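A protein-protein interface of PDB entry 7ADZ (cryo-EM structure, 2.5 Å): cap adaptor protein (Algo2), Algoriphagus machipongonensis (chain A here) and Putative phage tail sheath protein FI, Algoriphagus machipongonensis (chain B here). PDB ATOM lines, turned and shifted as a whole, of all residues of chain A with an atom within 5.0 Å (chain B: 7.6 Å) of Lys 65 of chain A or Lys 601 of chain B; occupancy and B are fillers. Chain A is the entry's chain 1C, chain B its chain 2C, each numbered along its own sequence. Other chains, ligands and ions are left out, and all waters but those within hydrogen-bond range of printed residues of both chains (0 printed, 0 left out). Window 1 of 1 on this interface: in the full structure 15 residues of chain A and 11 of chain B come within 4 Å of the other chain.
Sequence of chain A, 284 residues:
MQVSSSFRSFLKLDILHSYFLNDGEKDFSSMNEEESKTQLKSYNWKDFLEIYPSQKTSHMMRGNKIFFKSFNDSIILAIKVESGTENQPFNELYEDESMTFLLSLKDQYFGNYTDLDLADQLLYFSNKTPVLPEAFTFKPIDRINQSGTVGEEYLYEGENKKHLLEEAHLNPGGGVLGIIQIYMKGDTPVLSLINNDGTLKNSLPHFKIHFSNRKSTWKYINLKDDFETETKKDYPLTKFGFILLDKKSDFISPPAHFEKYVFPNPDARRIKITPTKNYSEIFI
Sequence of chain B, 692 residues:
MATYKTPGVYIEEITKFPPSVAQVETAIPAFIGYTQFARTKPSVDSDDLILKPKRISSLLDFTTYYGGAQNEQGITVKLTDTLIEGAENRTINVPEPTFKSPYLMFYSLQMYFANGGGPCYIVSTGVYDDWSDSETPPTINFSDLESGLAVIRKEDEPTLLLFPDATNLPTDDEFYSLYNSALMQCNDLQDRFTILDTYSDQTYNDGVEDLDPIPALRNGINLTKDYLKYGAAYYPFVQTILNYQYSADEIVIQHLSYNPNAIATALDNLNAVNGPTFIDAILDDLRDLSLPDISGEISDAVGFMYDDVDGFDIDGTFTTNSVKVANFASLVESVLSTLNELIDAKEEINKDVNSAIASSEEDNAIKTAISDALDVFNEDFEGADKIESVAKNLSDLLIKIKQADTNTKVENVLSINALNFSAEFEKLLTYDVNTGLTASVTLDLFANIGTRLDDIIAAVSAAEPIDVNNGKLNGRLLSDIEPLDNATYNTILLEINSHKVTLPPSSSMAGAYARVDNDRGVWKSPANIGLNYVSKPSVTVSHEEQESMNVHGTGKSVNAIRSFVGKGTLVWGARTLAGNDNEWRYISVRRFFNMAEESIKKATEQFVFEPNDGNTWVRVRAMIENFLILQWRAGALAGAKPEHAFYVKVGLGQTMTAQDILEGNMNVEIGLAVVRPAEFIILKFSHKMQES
Printed residues of chain B within 4 Å of Lys 65 of chain A: Lys 601 (3.5 Å).
Of chain A, only Lys 65 (3.5 Å) comes within 4 Å of Lys 601 of chain B.
Of the printed residues of chain B, Asn 91 of chain A touches Arg 153.
Printed residues of chain A within 4 Å of Asp 156 of chain B: Arg 62.
Of the printed residues of chain B, Phe 67 of chain A touches Glu 605.
Of the printed residues of chain A, Arg 153 of chain B touches Asn 91 (3.8 Å).
The nearest printed residue of chain A that does not touch Lys 601 of chain B is Lys 80 of chain A (6.1 Å).
Of the 12 printed residues of chain A, 6 touch a printed residue of chain B.
Hydrophobic or aromatic side chains of chain A that line the printed part of chain B: Phe 67.
Among the printed residues, 6 pairs touch across the chains.
Among the printed residues, Asp or Glu carboxylates within 4 Å of a Lys or Arg side-chain nitrogen of the other chain: Arg 62 of chain A with Asp 156 of chain B (3.5 Å).
NE of Arg 62 of chain A is in salt-bridge range of OD2 of Asp 156 of chain B (3.5 Å).
The backbone carbonyl oxygen (O) of Ala 78 of chain A lies within hydrogen-bond range of the backbone NH (N) of Phe 67 of chain A, 2.8 Å away.
O of Lys 601 of chain B is in hydrogen-bond range of OG1 of Thr 604 of chain B (3.2 Å).
The backbone carbonyl oxygen (O) of Lys 65 of chain A lies within hydrogen-bond range of the backbone NH (N) of Lys 80 of chain A (3.2 Å).
ND2 of Asn 91 of chain A lies within hydrogen-bond range of O of Gly 63 of chain A (3.3 Å).
Among the printed residues, merely in contact across the chains: Gly 63 of chain A with Lys 154 of chain B (3.3 Å), Asn 64 of chain A with Lys 154 of chain B (3.6 Å), Lys 65 of chain A with Lys 601 of chain B (3.5 Å), Phe 67 of chain A with Glu 605 of chain B (3.97 Å) and Asn 91 of chain A with Arg 153 of chain B (3.8 Å).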
ATOM      1  N   MET A  60       3.367   8.198 -14.932  1.00  0.00           N
ATOM      2  CA  MET A  60       3.552   7.254 -16.020  1.00  0.00           C
ATOM      3  C   MET A  60       3.227   7.888 -17.366  1.00  0.00           C
ATOM      4  O   MET A  60       3.989   7.730 -18.323  1.00  0.00           O
ATOM      5  CB  MET A  60       2.639   6.048 -15.906  1.00  0.00           C
ATOM      6  CG  MET A  60       2.928   4.995 -16.995  1.00  0.00           C
ATOM      7  SD  MET A  60       1.662   3.790 -17.233  1.00  0.00           S
ATOM      8  CE  MET A  60       0.637   4.709 -18.353  1.00  0.00           C
ATOM      9  N   MET A  61       2.092   8.597 -17.450  1.00  0.00           N
ATOM     10  CA  MET A  61       1.669   9.194 -18.703  1.00  0.00           C
ATOM     11  C   MET A  61       2.720  10.164 -19.201  1.00  0.00           C
ATOM     12  O   MET A  61       2.981  10.231 -20.404  1.00  0.00           O
ATOM     13  CB  MET A  61       0.305   9.866 -18.561  1.00  0.00           C
ATOM     14  CG  MET A  61      -0.872   8.896 -18.370  1.00  0.00           C
ATOM     15  SD  MET A  61      -2.452   9.728 -18.047  1.00  0.00           S
ATOM     16  CE  MET A  61      -2.981  10.302 -19.635  1.00  0.00           C
ATOM     17  N   ARG A  62       3.349  10.929 -18.304  1.00  0.00           N
ATOM     18  CA  ARG A  62       4.409  11.798 -18.774  1.00  0.00           C
ATOM     19  C   ARG A  62       5.540  10.976 -19.383  1.00  0.00           C
ATOM     20  O   ARG A  62       5.980  11.235 -20.504  1.00  0.00           O
ATOM     21  CB  ARG A  62       4.986  12.636 -17.643  1.00  0.00           C
ATOM     22  CG  ARG A  62       4.136  13.795 -17.145  1.00  0.00           C
ATOM     23  CD  ARG A  62       4.943  14.678 -16.252  1.00  0.00           C
ATOM     24  NE  ARG A  62       5.258  14.029 -14.963  1.00  0.00           N
ATOM     25  CZ  ARG A  62       4.522  14.141 -13.818  1.00  0.00           C
ATOM     26  NH1 ARG A  62       3.451  14.908 -13.790  1.00  0.00           N
ATOM     27  NH2 ARG A  62       4.870  13.481 -12.710  1.00  0.00           N
ATOM     28  N   GLY A  63       5.969   9.925 -18.687  1.00  0.00           N
ATOM     29  CA  GLY A  63       7.068   9.092 -19.162  1.00  0.00           C
ATOM     30  C   GLY A  63       6.807   8.416 -20.503  1.00  0.00           C
ATOM     31  O   GLY A  63       7.696   8.338 -21.350  1.00  0.00           O
ATOM     32  N   ASN A  64       5.577   7.963 -20.719  1.00  0.00           N
ATOM     33  CA  ASN A  64       5.214   7.286 -21.956  1.00  0.00           C
ATOM     34  C   ASN A  64       4.599   8.177 -23.021  1.00  0.00           C
ATOM     35  O   ASN A  64       4.146   7.661 -24.041  1.00  0.00           O
ATOM     36  CB  ASN A  64       4.265   6.132 -21.702  1.00  0.00           C
ATOM     37  CG  ASN A  64       4.889   4.954 -21.035  1.00  0.00           C
ATOM     38  OD1 ASN A  64       6.089   4.697 -21.158  1.00  0.00           O
ATOM     39  ND2 ASN A  64       4.070   4.205 -20.350  1.00  0.00           N
ATOM     40  N   LYS A  65       4.589   9.495 -22.822  1.00  0.00           N
ATOM     41  CA  LYS A  65       4.008  10.428 -23.780  1.00  0.00           C
ATOM     42  C   LYS A  65       2.531  10.175 -24.115  1.00  0.00           C
ATOM     43  O   LYS A  65       2.149  10.115 -25.294  1.00  0.00           O
ATOM     44  CB  LYS A  65       4.837  10.442 -25.059  1.00  0.00           C
ATOM     45  CG  LYS A  65       6.337  10.652 -24.840  1.00  0.00           C
ATOM     46  CD  LYS A  65       6.652  12.018 -24.238  1.00  0.00           C
ATOM     47  CE  LYS A  65       8.145  12.208 -24.080  1.00  0.00           C
ATOM     48  NZ  LYS A  65       8.486  13.519 -23.444  1.00  0.00           N
ATOM     49  N   ILE A  66       1.708  10.006 -23.075  1.00  0.00           N
ATOM     50  CA  ILE A  66       0.265   9.806 -23.233  1.00  0.00           C
ATOM     51  C   ILE A  66      -0.476  11.057 -22.737  1.00  0.00           C
ATOM     52  O   ILE A  66      -0.231  11.547 -21.640  1.00  0.00           O
ATOM     53  CB  ILE A  66      -0.238   8.538 -22.505  1.00  0.00           C
ATOM     54  CG1 ILE A  66       0.498   7.297 -23.068  1.00  0.00           C
ATOM     55  CG2 ILE A  66      -1.770   8.384 -22.752  1.00  0.00           C
ATOM     56  CD1 ILE A  66       0.316   6.017 -22.277  1.00  0.00           C
ATOM     57  N   PHE A  67      -1.369  11.583 -23.562  1.00  0.00           N
ATOM     58  CA  PHE A  67      -2.086  12.827 -23.279  1.00  0.00           C
ATOM     59  C   PHE A  67      -3.575  12.610 -23.048  1.00  0.00           C
ATOM     60  O   PHE A  67      -4.171  11.696 -23.614  1.00  0.00           O
ATOM     61  CB  PHE A  67      -1.873  13.763 -24.457  1.00  0.00           C
ATOM     62  CG  PHE A  67      -0.429  14.024 -24.651  1.00  0.00           C
ATOM     63  CD1 PHE A  67       0.305  13.179 -25.466  1.00  0.00           C
ATOM     64  CD2 PHE A  67       0.222  15.052 -24.013  1.00  0.00           C
ATOM     65  CE1 PHE A  67       1.635  13.351 -25.633  1.00  0.00           C
ATOM     66  CE2 PHE A  67       1.574  15.231 -24.192  1.00  0.00           C
ATOM     67  CZ  PHE A  67       2.280  14.373 -25.002  1.00  0.00           C
ATOM     68  N   ALA A  78      -4.437  10.133 -26.189  1.00  0.00           N
ATOM     69  CA  ALA A  78      -3.603  10.122 -27.395  1.00  0.00           C
ATOM     70  C   ALA A  78      -2.159   9.806 -27.054  1.00  0.00           C
ATOM     71  O   ALA A  78      -1.673  10.152 -25.982  1.00  0.00           O
ATOM     72  CB  ALA A  78      -3.690  11.455 -28.107  1.00  0.00           C
ATOM     73  N   ILE A  79      -1.463   9.168 -27.986  1.00  0.00           N
ATOM     74  CA  ILE A  79      -0.092   8.743 -27.733  1.00  0.00           C
ATOM     75  C   ILE A  79       0.910   9.157 -28.816  1.00  0.00           C
ATOM     76  O   ILE A  79       0.586   9.197 -30.005  1.00  0.00           O
ATOM     77  CB  ILE A  79      -0.119   7.198 -27.557  1.00  0.00           C
ATOM     78  CG1 ILE A  79       1.213   6.650 -27.067  1.00  0.00           C
ATOM     79  CG2 ILE A  79      -0.500   6.530 -28.907  1.00  0.00           C
ATOM     80  CD1 ILE A  79       1.125   5.223 -26.532  1.00  0.00           C
ATOM     81  N   LYS A  80       2.138   9.475 -28.403  1.00  0.00           N
ATOM     82  CA  LYS A  80       3.201   9.747 -29.374  1.00  0.00           C
ATOM     83  C   LYS A  80       3.630   8.465 -30.093  1.00  0.00           C
ATOM     84  O   LYS A  80       3.915   7.448 -29.442  1.00  0.00           O
ATOM     85  CB  LYS A  80       4.417  10.381 -28.705  1.00  0.00           C
ATOM     86  CG  LYS A  80       5.525  10.784 -29.670  1.00  0.00           C
ATOM     87  CD  LYS A  80       6.660  11.510 -28.971  1.00  0.00           C
ATOM     88  CE  LYS A  80       7.808  11.762 -29.928  1.00  0.00           C
ATOM     89  NZ  LYS A  80       8.899  12.550 -29.305  1.00  0.00           N
ATOM     90  N   ASN A  91       7.484   4.809 -27.293  1.00  0.00           N
ATOM     91  CA  ASN A  91       8.053   3.989 -26.229  1.00  0.00           C
ATOM     92  C   ASN A  91       7.353   2.639 -26.180  1.00  0.00           C
ATOM     93  O   ASN A  91       6.138   2.568 -26.331  1.00  0.00           O
ATOM     94  CB  ASN A  91       7.955   4.678 -24.889  1.00  0.00           C
ATOM     95  CG  ASN A  91       8.849   5.852 -24.779  1.00  0.00           C
ATOM     96  OD1 ASN A  91      10.033   5.784 -25.117  1.00  0.00           O
ATOM     97  ND2 ASN A  91       8.316   6.934 -24.317  1.00  0.00           N
ATOM     98  N   ARG B 153      14.767   4.410 -20.272  1.00  0.00           N
ATOM     99  CA  ARG B 153      14.260   5.138 -21.417  1.00  0.00           C
ATOM    100  C   ARG B 153      12.871   5.698 -21.167  1.00  0.00           C
ATOM    101  O   ARG B 153      12.482   6.691 -21.776  1.00  0.00           O
ATOM    102  CB  ARG B 153      14.241   4.290 -22.664  1.00  0.00           C
ATOM    103  CG  ARG B 153      13.839   5.065 -23.900  1.00  0.00           C
ATOM    104  CD  ARG B 153      14.134   4.362 -25.137  1.00  0.00           C
ATOM    105  NE  ARG B 153      13.594   5.092 -26.276  1.00  0.00           N
ATOM    106  CZ  ARG B 153      13.961   4.936 -27.561  1.00  0.00           C
ATOM    107  NH1 ARG B 153      14.910   4.088 -27.890  1.00  0.00           N
ATOM    108  NH2 ARG B 153      13.365   5.648 -28.499  1.00  0.00           N
ATOM    109  N   LYS B 154      12.090   5.053 -20.304  1.00  0.00           N
ATOM    110  CA  LYS B 154      10.744   5.509 -20.045  1.00  0.00           C
ATOM    111  C   LYS B 154      10.628   6.568 -18.954  1.00  0.00           C
ATOM    112  O   LYS B 154       9.513   6.988 -18.649  1.00  0.00           O
ATOM    113  CB  LYS B 154       9.851   4.336 -19.690  1.00  0.00           C
ATOM    114  CG  LYS B 154       9.625   3.363 -20.812  1.00  0.00           C
ATOM    115  CD  LYS B 154       8.685   2.264 -20.374  1.00  0.00           C
ATOM    116  CE  LYS B 154       8.404   1.296 -21.485  1.00  0.00           C
ATOM    117  NZ  LYS B 154       7.491   0.220 -21.048  1.00  0.00           N
ATOM    118  N   GLU B 155      11.738   6.983 -18.341  1.00  0.00           N
ATOM    119  CA  GLU B 155      11.647   7.998 -17.301  1.00  0.00           C
ATOM    120  C   GLU B 155      11.832   9.375 -17.903  1.00  0.00           C
ATOM    121  O   GLU B 155      12.610   9.563 -18.836  1.00  0.00           O
ATOM    122  CB  GLU B 155      12.658   7.737 -16.191  1.00  0.00           C
ATOM    123  CG  GLU B 155      12.404   6.460 -15.442  1.00  0.00           C
ATOM    124  CD  GLU B 155      11.151   6.530 -14.677  1.00  0.00           C
ATOM    125  OE1 GLU B 155      10.867   7.583 -14.178  1.00  0.00           O
ATOM    126  OE2 GLU B 155      10.455   5.553 -14.609  1.00  0.00           O
ATOM    127  N   ASP B 156      11.136  10.351 -17.361  1.00  0.00           N
ATOM    128  CA  ASP B 156      11.204  11.731 -17.802  1.00  0.00           C
ATOM    129  C   ASP B 156      12.305  12.588 -17.178  1.00  0.00           C
ATOM    130  O   ASP B 156      13.033  13.282 -17.879  1.00  0.00           O
ATOM    131  CB  ASP B 156       9.831  12.344 -17.608  1.00  0.00           C
ATOM    132  CG  ASP B 156       9.322  12.101 -16.206  1.00  0.00           C
ATOM    133  OD1 ASP B 156      10.039  11.453 -15.438  1.00  0.00           O
ATOM    134  OD2 ASP B 156       8.246  12.522 -15.898  1.00  0.00           O
ATOM    135  N   LEU B 189      16.466  10.509 -28.081  1.00  0.00           N
ATOM    136  CA  LEU B 189      15.657  11.374 -27.219  1.00  0.00           C
ATOM    137  C   LEU B 189      15.930  12.887 -27.351  1.00  0.00           C
ATOM    138  O   LEU B 189      15.014  13.691 -27.190  1.00  0.00           O
ATOM    139  CB  LEU B 189      15.867  10.940 -25.768  1.00  0.00           C
ATOM    140  CG  LEU B 189      15.442   9.477 -25.400  1.00  0.00           C
ATOM    141  CD1 LEU B 189      15.860   9.200 -23.972  1.00  0.00           C
ATOM    142  CD2 LEU B 189      13.946   9.280 -25.559  1.00  0.00           C
ATOM    143  N   GLN B 190      17.173  13.270 -27.669  1.00  0.00           N
ATOM    144  CA  GLN B 190      17.646  14.658 -27.812  1.00  0.00           C
ATOM    145  C   GLN B 190      17.655  15.521 -26.542  1.00  0.00           C
ATOM    146  O   GLN B 190      17.651  16.745 -26.647  1.00  0.00           O
ATOM    147  CB  GLN B 190      16.814  15.421 -28.868  1.00  0.00           C
ATOM    148  CG  GLN B 190      16.849  14.863 -30.281  1.00  0.00           C
ATOM    149  CD  GLN B 190      18.176  15.096 -30.973  1.00  0.00           C
ATOM    150  OE1 GLN B 190      18.603  16.244 -31.167  1.00  0.00           O
ATOM    151  NE2 GLN B 190      18.829  14.005 -31.337  1.00  0.00           N
ATOM    152  N   ASP B 191      17.732  14.923 -25.353  1.00  0.00           N
ATOM    153  CA  ASP B 191      17.798  15.678 -24.109  1.00  0.00           C
ATOM    154  C   ASP B 191      18.705  15.094 -23.001  1.00  0.00           C
ATOM    155  O   ASP B 191      18.627  15.530 -21.854  1.00  0.00           O
ATOM    156  CB  ASP B 191      16.386  15.810 -23.594  1.00  0.00           C
ATOM    157  CG  ASP B 191      15.810  14.440 -23.393  1.00  0.00           C
ATOM    158  OD1 ASP B 191      16.509  13.490 -23.737  1.00  0.00           O
ATOM    159  OD2 ASP B 191      14.702  14.316 -22.916  1.00  0.00           O
ATOM    160  N   MET B 595      18.706  21.901 -22.073  1.00  0.00           N
ATOM    161  CA  MET B 595      17.856  22.539 -21.078  1.00  0.00           C
ATOM    162  C   MET B 595      16.774  23.387 -21.737  1.00  0.00           C
ATOM    163  O   MET B 595      15.590  23.301 -21.387  1.00  0.00           O
ATOM    164  CB  MET B 595      18.732  23.390 -20.160  1.00  0.00           C
ATOM    165  CG  MET B 595      18.038  24.168 -19.030  1.00  0.00           C
ATOM    166  SD  MET B 595      17.314  25.767 -19.564  1.00  0.00           S
ATOM    167  CE  MET B 595      18.701  26.794 -19.998  1.00  0.00           C
ATOM    168  N   ALA B 596      17.174  24.223 -22.696  1.00  0.00           N
ATOM    169  CA  ALA B 596      16.216  25.078 -23.361  1.00  0.00           C
ATOM    170  C   ALA B 596      15.156  24.258 -24.082  1.00  0.00           C
ATOM    171  O   ALA B 596      13.970  24.602 -24.025  1.00  0.00           O
ATOM    172  CB  ALA B 596      16.931  25.999 -24.328  1.00  0.00           C
ATOM    173  N   GLU B 597      15.558  23.139 -24.702  1.00  0.00           N
ATOM    174  CA  GLU B 597      14.604  22.308 -25.415  1.00  0.00           C
ATOM    175  C   GLU B 597      13.595  21.696 -24.471  1.00  0.00           C
ATOM    176  O   GLU B 597      12.402  21.685 -24.763  1.00  0.00           O
ATOM    177  CB  GLU B 597      15.310  21.200 -26.188  1.00  0.00           C
ATOM    178  CG  GLU B 597      14.378  20.264 -26.989  1.00  0.00           C
ATOM    179  CD  GLU B 597      13.627  20.951 -28.103  1.00  0.00           C
ATOM    180  OE1 GLU B 597      14.037  22.015 -28.513  1.00  0.00           O
ATOM    181  OE2 GLU B 597      12.649  20.404 -28.551  1.00  0.00           O
ATOM    182  N   GLU B 598      14.008  21.225 -23.299  1.00  0.00           N
ATOM    183  CA  GLU B 598      13.001  20.651 -22.421  1.00  0.00           C
ATOM    184  C   GLU B 598      11.875  21.642 -22.132  1.00  0.00           C
ATOM    185  O   GLU B 598      10.693  21.281 -22.187  1.00  0.00           O
ATOM    186  CB  GLU B 598      13.601  20.185 -21.101  1.00  0.00           C
ATOM    187  CG  GLU B 598      12.559  19.570 -20.160  1.00  0.00           C
ATOM    188  CD  GLU B 598      13.105  19.097 -18.858  1.00  0.00           C
ATOM    189  OE1 GLU B 598      14.294  19.094 -18.688  1.00  0.00           O
ATOM    190  OE2 GLU B 598      12.308  18.755 -18.007  1.00  0.00           O
ATOM    191  N   SER B 599      12.230  22.889 -21.811  1.00  0.00           N
ATOM    192  CA  SER B 599      11.208  23.885 -21.497  1.00  0.00           C
ATOM    193  C   SER B 599      10.325  24.251 -22.684  1.00  0.00           C
ATOM    194  O   SER B 599       9.099  24.359 -22.553  1.00  0.00           O
ATOM    195  CB  SER B 599      11.854  25.139 -20.963  1.00  0.00           C
ATOM    196  OG  SER B 599      12.450  24.918 -19.718  1.00  0.00           O
ATOM    197  N   ILE B 600      10.933  24.423 -23.849  1.00  0.00           N
ATOM    198  CA  ILE B 600      10.173  24.791 -25.027  1.00  0.00           C
ATOM    199  C   ILE B 600       9.240  23.660 -25.415  1.00  0.00           C
ATOM    200  O   ILE B 600       8.073  23.901 -25.718  1.00  0.00           O
ATOM    201  CB  ILE B 600      11.100  25.254 -26.150  1.00  0.00           C
ATOM    202  CG1 ILE B 600      11.737  26.604 -25.676  1.00  0.00           C
ATOM    203  CG2 ILE B 600      10.309  25.418 -27.465  1.00  0.00           C
ATOM    204  CD1 ILE B 600      12.899  27.097 -26.470  1.00  0.00           C
ATOM    205  N   LYS B 601       9.727  22.432 -25.412  1.00  0.00           N
ATOM    206  CA  LYS B 601       8.868  21.314 -25.721  1.00  0.00           C
ATOM    207  C   LYS B 601       7.610  21.329 -24.858  1.00  0.00           C
ATOM    208  O   LYS B 601       6.500  21.285 -25.389  1.00  0.00           O
ATOM    209  CB  LYS B 601       9.636  20.011 -25.548  1.00  0.00           C
ATOM    210  CG  LYS B 601       8.829  18.754 -25.801  1.00  0.00           C
ATOM    211  CD  LYS B 601       9.702  17.493 -25.801  1.00  0.00           C
ATOM    212  CE  LYS B 601      10.322  17.208 -24.438  1.00  0.00           C
ATOM    213  NZ  LYS B 601      10.943  15.858 -24.391  1.00  0.00           N
ATOM    214  N   LYS B 602       7.755  21.481 -23.537  1.00  0.00           N
ATOM    215  CA  LYS B 602       6.571  21.499 -22.676  1.00  0.00           C
ATOM    216  C   LYS B 602       5.590  22.593 -23.094  1.00  0.00           C
ATOM    217  O   LYS B 602       4.372  22.408 -23.059  1.00  0.00           O
ATOM    218  CB  LYS B 602       6.985  21.676 -21.222  1.00  0.00           C
ATOM    219  CG  LYS B 602       7.651  20.453 -20.635  1.00  0.00           C
ATOM    220  CD  LYS B 602       8.125  20.670 -19.201  1.00  0.00           C
ATOM    221  CE  LYS B 602       8.790  19.402 -18.663  1.00  0.00           C
ATOM    222  NZ  LYS B 602       9.383  19.593 -17.312  1.00  0.00           N
ATOM    223  N   ALA B 603       6.115  23.751 -23.486  1.00  0.00           N
ATOM    224  CA  ALA B 603       5.285  24.854 -23.954  1.00  0.00           C
ATOM    225  C   ALA B 603       4.470  24.512 -25.210  1.00  0.00           C
ATOM    226  O   ALA B 603       3.359  25.019 -25.369  1.00  0.00           O
ATOM    227  CB  ALA B 603       6.144  26.079 -24.255  1.00  0.00           C
ATOM    228  N   THR B 604       4.994  23.688 -26.128  1.00  0.00           N
ATOM    229  CA  THR B 604       4.235  23.445 -27.353  1.00  0.00           C
ATOM    230  C   THR B 604       3.331  22.217 -27.258  1.00  0.00           C
ATOM    231  O   THR B 604       2.288  22.168 -27.913  1.00  0.00           O
ATOM    232  CB  THR B 604       5.162  23.325 -28.595  1.00  0.00           C
ATOM    233  OG1 THR B 604       6.034  22.204 -28.461  1.00  0.00           O
ATOM    234  CG2 THR B 604       6.012  24.592 -28.732  1.00  0.00           C
ATOM    235  N   GLU B 605       3.637  21.284 -26.354  1.00  0.00           N
ATOM    236  CA  GLU B 605       2.827  20.068 -26.172  1.00  0.00           C
ATOM    237  C   GLU B 605       1.416  20.367 -25.671  1.00  0.00           C
ATOM    238  O   GLU B 605       0.496  19.566 -25.832  1.00  0.00           O
ATOM    239  CB  GLU B 605       3.514  19.048 -25.272  1.00  0.00           C
ATOM    240  CG  GLU B 605       4.714  18.354 -25.924  1.00  0.00           C
ATOM    241  CD  GLU B 605       5.372  17.313 -25.046  1.00  0.00           C
ATOM    242  OE1 GLU B 605       5.011  17.201 -23.898  1.00  0.00           O
ATOM    243  OE2 GLU B 605       6.231  16.618 -25.540  1.00  0.00           O
ATOM    244  N   GLN B 606       1.223  21.535 -25.099  1.00  0.00           N
ATOM    245  CA  GLN B 606      -0.079  21.938 -24.596  1.00  0.00           C
ATOM    246  C   GLN B 606      -1.107  22.095 -25.715  1.00  0.00           C
ATOM    247  O   GLN B 606      -2.304  22.164 -25.450  1.00  0.00           O
ATOM    248  CB  GLN B 606       0.022  23.244 -23.820  1.00  0.00           C
ATOM    249  CG  GLN B 606       0.775  23.119 -22.523  1.00  0.00           C
ATOM    250  CD  GLN B 606       0.853  24.411 -21.764  1.00  0.00           C
ATOM    251  OE1 GLN B 606       0.073  25.339 -22.002  1.00  0.00           O
ATOM    252  NE2 GLN B 606       1.796  24.489 -20.838  1.00  0.00           N
ATOM    253  N   PHE B 607      -0.651  22.166 -26.961  1.00  0.00           N
ATOM    254  CA  PHE B 607      -1.520  22.377 -28.093  1.00  0.00           C
ATOM    255  C   PHE B 607      -1.724  21.155 -28.995  1.00  0.00           C
ATOM    256  O   PHE B 607      -2.163  21.318 -30.135  1.00  0.00           O
ATOM    257  CB  PHE B 607      -0.952  23.538 -28.899  1.00  0.00           C
ATOM    258  CG  PHE B 607      -0.881  24.789 -28.092  1.00  0.00           C
ATOM    259  CD1 PHE B 607       0.294  25.147 -27.476  1.00  0.00           C
ATOM    260  CD2 PHE B 607      -1.973  25.603 -27.925  1.00  0.00           C
ATOM    261  CE1 PHE B 607       0.380  26.277 -26.717  1.00  0.00           C
ATOM    262  CE2 PHE B 607      -1.891  26.747 -27.173  1.00  0.00           C
ATOM    263  CZ  PHE B 607      -0.712  27.084 -26.566  1.00  0.00           C
ATOM    264  N   ILE B 624       7.027  31.068 -25.549  1.00  0.00           N
ATOM    265  CA  ILE B 624       8.431  30.836 -25.814  1.00  0.00           C
ATOM    266  C   ILE B 624       9.255  32.084 -25.555  1.00  0.00           C
ATOM    267  O   ILE B 624      10.327  31.994 -24.947  1.00  0.00           O
ATOM    268  CB  ILE B 624       8.661  30.322 -27.234  1.00  0.00           C
ATOM    269  CG1 ILE B 624       8.016  28.936 -27.364  1.00  0.00           C
ATOM    270  CG2 ILE B 624      10.192  30.229 -27.504  1.00  0.00           C
ATOM    271  CD1 ILE B 624       7.889  28.429 -28.766  1.00  0.00           C
